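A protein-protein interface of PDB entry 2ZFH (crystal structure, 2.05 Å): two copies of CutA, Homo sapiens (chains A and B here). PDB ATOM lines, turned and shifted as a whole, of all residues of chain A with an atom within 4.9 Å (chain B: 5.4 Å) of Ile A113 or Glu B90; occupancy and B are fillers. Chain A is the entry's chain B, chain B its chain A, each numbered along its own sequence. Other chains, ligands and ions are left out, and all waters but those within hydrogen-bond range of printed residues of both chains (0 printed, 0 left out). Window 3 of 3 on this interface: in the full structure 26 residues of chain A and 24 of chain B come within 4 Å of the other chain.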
ATOM      1  N   ILE A 106      -1.336  14.031 -24.356  1.00  0.00           N
ATOM      2  CA  ILE A 106      -0.686  15.090 -23.606  1.00  0.00           C
ATOM      3  C   ILE A 106      -1.425  15.183 -22.283  1.00  0.00           C
ATOM      4  O   ILE A 106      -2.614  15.493 -22.250  1.00  0.00           O
ATOM      5  CB  ILE A 106      -0.770  16.435 -24.370  1.00  0.00           C
ATOM      6  CG1 ILE A 106       0.039  16.330 -25.667  1.00  0.00           C
ATOM      7  CG2 ILE A 106      -0.259  17.575 -23.500  1.00  0.00           C
ATOM      8  CD1 ILE A 106      -0.045  17.550 -26.556  1.00  0.00           C
ATOM      9  N   TYR A 107      -0.719  14.904 -21.194  1.00  0.00           N
ATOM     10  CA  TYR A 107      -1.325  14.925 -19.874  1.00  0.00           C
ATOM     11  C   TYR A 107      -0.327  15.340 -18.815  1.00  0.00           C
ATOM     12  O   TYR A 107       0.875  15.424 -19.071  1.00  0.00           O
ATOM     13  CB  TYR A 107      -1.827  13.536 -19.523  1.00  0.00           C
ATOM     14  CG  TYR A 107      -0.723  12.508 -19.570  1.00  0.00           C
ATOM     15  CD1 TYR A 107      -0.259  12.013 -20.790  1.00  0.00           C
ATOM     16  CD2 TYR A 107      -0.122  12.046 -18.395  1.00  0.00           C
ATOM     17  CE1 TYR A 107       0.772  11.080 -20.844  1.00  0.00           C
ATOM     18  CE2 TYR A 107       0.911  11.116 -18.432  1.00  0.00           C
ATOM     19  CZ  TYR A 107       1.355  10.634 -19.661  1.00  0.00           C
ATOM     20  OH  TYR A 107       2.373   9.705 -19.709  1.00  0.00           O
ATOM     21  N   GLU A 108      -0.831  15.574 -17.611  1.00  0.00           N
ATOM     22  CA  GLU A 108       0.027  15.964 -16.507  1.00  0.00           C
ATOM     23  C   GLU A 108       0.522  14.703 -15.815  1.00  0.00           C
ATOM     24  O   GLU A 108      -0.134  13.661 -15.843  1.00  0.00           O
ATOM     25  CB  GLU A 108      -0.742  16.820 -15.501  1.00  0.00           C
ATOM     26  CG  GLU A 108       0.134  17.779 -14.699  1.00  0.00           C
ATOM     27  CD  GLU A 108       0.390  19.095 -15.431  1.00  0.00           C
ATOM     28  OE1 GLU A 108       0.948  19.067 -16.549  1.00  0.00           O
ATOM     29  OE2 GLU A 108       0.028  20.161 -14.887  1.00  0.00           O
ATOM     30  N   GLY A 111       2.983  16.924 -11.758  1.00  0.00           N
ATOM     31  CA  GLY A 111       3.107  18.347 -12.012  1.00  0.00           C
ATOM     32  C   GLY A 111       3.658  18.746 -13.369  1.00  0.00           C
ATOM     33  O   GLY A 111       3.438  19.874 -13.815  1.00  0.00           O
ATOM     34  N   LYS A 112       4.366  17.838 -14.034  1.00  0.00           N
ATOM     35  CA  LYS A 112       4.943  18.139 -15.342  1.00  0.00           C
ATOM     36  C   LYS A 112       4.110  17.626 -16.515  1.00  0.00           C
ATOM     37  O   LYS A 112       3.488  16.566 -16.437  1.00  0.00           O
ATOM     38  CB  LYS A 112       6.356  17.554 -15.457  1.00  0.00           C
ATOM     39  CG  LYS A 112       7.441  18.292 -14.693  1.00  0.00           C
ATOM     40  CD  LYS A 112       7.337  18.062 -13.202  1.00  0.00           C
ATOM     41  CE  LYS A 112       8.535  18.656 -12.475  1.00  0.00           C
ATOM     42  NZ  LYS A 112       8.418  18.458 -11.008  1.00  0.00           N
ATOM     43  N   ILE A 113       4.129  18.376 -17.612  1.00  0.00           N
ATOM     44  CA  ILE A 113       3.396  18.009 -18.811  1.00  0.00           C
ATOM     45  C   ILE A 113       4.170  16.962 -19.597  1.00  0.00           C
ATOM     46  O   ILE A 113       5.365  17.100 -19.835  1.00  0.00           O
ATOM     47  CB  ILE A 113       3.144  19.238 -19.695  1.00  0.00           C
ATOM     48  CG1 ILE A 113       2.298  20.250 -18.918  1.00  0.00           C
ATOM     49  CG2 ILE A 113       2.432  18.824 -20.978  1.00  0.00           C
ATOM     50  CD1 ILE A 113       2.021  21.531 -19.660  1.00  0.00           C
ATOM     51  N   GLU A 114       3.481  15.908 -20.009  1.00  0.00           N
ATOM     52  CA  GLU A 114       4.133  14.840 -20.742  1.00  0.00           C
ATOM     53  C   GLU A 114       3.441  14.568 -22.077  1.00  0.00           C
ATOM     54  O   GLU A 114       2.270  14.899 -22.253  1.00  0.00           O
ATOM     55  CB  GLU A 114       4.143  13.584 -19.875  1.00  0.00           C
ATOM     56  CG  GLU A 114       5.216  12.592 -20.251  1.00  0.00           C
ATOM     57  CD  GLU A 114       5.446  11.555 -19.173  1.00  0.00           C
ATOM     58  OE1 GLU A 114       5.704  11.954 -18.017  1.00  0.00           O
ATOM     59  OE2 GLU A 114       5.375  10.347 -19.486  1.00  0.00           O
ATOM     60  N   GLU A 115       4.176  13.978 -23.015  1.00  0.00           N
ATOM     61  CA  GLU A 115       3.641  13.649 -24.331  1.00  0.00           C
ATOM     62  C   GLU A 115       3.992  12.217 -24.716  1.00  0.00           C
ATOM     63  O   GLU A 115       5.166  11.857 -24.787  1.00  0.00           O
ATOM     64  CB  GLU A 115       4.192  14.603 -25.391  1.00  0.00           C
ATOM     65  CG  GLU A 115       3.614  16.002 -25.331  1.00  0.00           C
ATOM     66  CD  GLU A 115       4.156  16.910 -26.425  1.00  0.00           C
ATOM     67  OE1 GLU A 115       4.155  16.493 -27.607  1.00  0.00           O
ATOM     68  OE2 GLU A 115       4.577  18.046 -26.101  1.00  0.00           O
ATOM     69  N   ALA B  85      -3.317  22.042 -26.689  1.00  0.00           N
ATOM     70  CA  ALA B  85      -3.341  20.906 -25.781  1.00  0.00           C
ATOM     71  C   ALA B  85      -2.450  21.135 -24.569  1.00  0.00           C
ATOM     72  O   ALA B  85      -2.866  20.897 -23.431  1.00  0.00           O
ATOM     73  CB  ALA B  85      -2.907  19.637 -26.509  1.00  0.00           C
ATOM     74  N   ARG B  86      -1.226  21.593 -24.814  1.00  0.00           N
ATOM     75  CA  ARG B  86      -0.279  21.845 -23.733  1.00  0.00           C
ATOM     76  C   ARG B  86      -0.783  22.968 -22.840  1.00  0.00           C
ATOM     77  O   ARG B  86      -0.727  22.873 -21.615  1.00  0.00           O
ATOM     78  CB  ARG B  86       1.104  22.201 -24.297  1.00  0.00           C
ATOM     79  CG  ARG B  86       1.616  21.201 -25.335  1.00  0.00           C
ATOM     80  CD  ARG B  86       3.056  21.455 -25.769  1.00  0.00           C
ATOM     81  NE  ARG B  86       3.989  20.609 -25.033  1.00  0.00           N
ATOM     82  CZ  ARG B  86       4.498  20.904 -23.840  1.00  0.00           C
ATOM     83  NH1 ARG B  86       4.178  22.043 -23.233  1.00  0.00           N
ATOM     84  NH2 ARG B  86       5.307  20.045 -23.238  1.00  0.00           N
ATOM     85  N   ALA B  87      -1.297  24.022 -23.456  1.00  0.00           N
ATOM     86  CA  ALA B  87      -1.807  25.156 -22.703  1.00  0.00           C
ATOM     87  C   ALA B  87      -2.978  24.784 -21.788  1.00  0.00           C
ATOM     88  O   ALA B  87      -2.976  25.130 -20.609  1.00  0.00           O
ATOM     89  CB  ALA B  87      -2.221  26.261 -23.660  1.00  0.00           C
ATOM     90  N   VAL B  88      -3.979  24.080 -22.314  1.00  0.00           N
ATOM     91  CA  VAL B  88      -5.127  23.716 -21.488  1.00  0.00           C
ATOM     92  C   VAL B  88      -4.753  22.764 -20.357  1.00  0.00           C
ATOM     93  O   VAL B  88      -5.346  22.813 -19.282  1.00  0.00           O
ATOM     94  CB  VAL B  88      -6.268  23.082 -22.324  1.00  0.00           C
ATOM     95  CG1 VAL B  88      -6.683  24.034 -23.429  1.00  0.00           C
ATOM     96  CG2 VAL B  88      -5.828  21.750 -22.901  1.00  0.00           C
ATOM     97  N   VAL B  89      -3.772  21.899 -20.594  1.00  0.00           N
ATOM     98  CA  VAL B  89      -3.340  20.962 -19.565  1.00  0.00           C
ATOM     99  C   VAL B  89      -2.523  21.681 -18.493  1.00  0.00           C
ATOM    100  O   VAL B  89      -2.612  21.364 -17.308  1.00  0.00           O
ATOM    101  CB  VAL B  89      -2.488  19.825 -20.160  1.00  0.00           C
ATOM    102  CG1 VAL B  89      -1.957  18.938 -19.053  1.00  0.00           C
ATOM    103  CG2 VAL B  89      -3.331  18.999 -21.130  1.00  0.00           C
ATOM    104  N   GLU B  90      -1.723  22.655 -18.906  1.00  0.00           N
ATOM    105  CA  GLU B  90      -0.917  23.391 -17.945  1.00  0.00           C
ATOM    106  C   GLU B  90      -1.822  24.277 -17.083  1.00  0.00           C
ATOM    107  O   GLU B  90      -1.602  24.416 -15.875  1.00  0.00           O
ATOM    108  CB  GLU B  90       0.117  24.254 -18.668  1.00  0.00           C
ATOM    109  CG  GLU B  90       1.232  24.733 -17.760  1.00  0.00           C
ATOM    110  CD  GLU B  90       1.812  26.060 -18.204  1.00  0.00           C
ATOM    111  OE1 GLU B  90       1.046  27.049 -18.257  1.00  0.00           O
ATOM    112  OE2 GLU B  90       3.030  26.116 -18.494  1.00  0.00           O
ATOM    113  N   LYS B  91      -2.842  24.864 -17.707  1.00  0.00           N
ATOM    114  CA  LYS B  91      -3.780  25.732 -16.999  1.00  0.00           C
ATOM    115  C   LYS B  91      -4.784  24.924 -16.181  1.00  0.00           C
ATOM    116  O   LYS B  91      -5.683  25.478 -15.544  1.00  0.00           O
ATOM    117  CB  LYS B  91      -4.526  26.627 -17.993  1.00  0.00           C
ATOM    118  CG  LYS B  91      -3.614  27.483 -18.863  1.00  0.00           C
ATOM    119  CD  LYS B  91      -4.407  28.514 -19.648  1.00  0.00           C
ATOM    120  CE  LYS B  91      -5.050  29.522 -18.709  1.00  0.00           C
ATOM    121  NZ  LYS B  91      -5.908  30.516 -19.414  1.00  0.00           N
ATOM    122  N   ARG B  92      -4.626  23.606 -16.210  1.00  0.00           N
ATOM    123  CA  ARG B  92      -5.499  22.703 -15.472  1.00  0.00           C
ATOM    124  C   ARG B  92      -6.980  22.765 -15.877  1.00  0.00           C
ATOM    125  O   ARG B  92      -7.870  22.469 -15.079  1.00  0.00           O
ATOM    126  CB  ARG B  92      -5.317  22.946 -13.970  1.00  0.00           C
ATOM    127  CG  ARG B  92      -3.943  22.477 -13.464  1.00  0.00           C
ATOM    128  CD  ARG B  92      -3.645  22.918 -12.031  1.00  0.00           C
ATOM    129  NE  ARG B  92      -4.516  22.292 -11.040  1.00  0.00           N
ATOM    130  CZ  ARG B  92      -4.316  21.092 -10.491  1.00  0.00           C
ATOM    131  NH1 ARG B  92      -3.256  20.357 -10.829  1.00  0.00           N
ATOM    132  NH2 ARG B  92      -5.183  20.632  -9.595  1.00  0.00           N
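NE of Arg B86 is in salt-bridge range of OE2 of Glu A115, at 2.8 Å.
O of Tyr A107 is in hydrogen-bond range of N of Glu A114. The side-chain carboxylate (OE1) of Glu A108 sits close to the backbone NH (N) of Ile A113, 3.4 Å away.
Ala B85 touches Ile A106 (CB to CD1, 3.5 Å). Val B89 touches Ile A106 (CG2 to O, 3.7 Å). Tyr A107 touches Val B89. Glu A108 touches Val B89. Arg B86 touches Ile A113. CD1 of Ile A113 touches CB of Glu B90 (3.5 Å).
Of chain B, only Arg B86 (3.6 Å) and Glu B90 (3.5 Å) come within 4 Å of Ile A113. Of chain A, only Ile A113 comes within 4 Å of Glu B90. Of the printed residues of chain B, Glu A108 touches Val B89. Printed residues of chain B within 4 Å of Glu A115: Arg B86. Of the printed residues of chain B, Ile A106 touches Ala B85 (3.5 Å) and Val B89 (3.7 Å). Of the printed residues of chain B, Tyr A107 touches Val B89 (3.96 Å). Arg B92 touches none of the printed residues of chain A. The nearest residue of chain A that does not touch Glu B90 is Glu A108 (4.5 Å).
Printed residues of chain B that touch a printed residue of chain A: Ala B85, Arg B86, Val B89 and Glu B90. Hydrophobic or aromatic side chains of chain B that line the printed part of chain A: Ala B85 and Val B89. Printed residues of chain A that touch a printed residue of chain B: Ile A106, Tyr A107, Glu A108, Ile A113 and Glu A115.
No position is printed for both chains. Of the 7 pairs that touch across the chains among the printed residues, none has its exchanged pair printed and touching as well.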
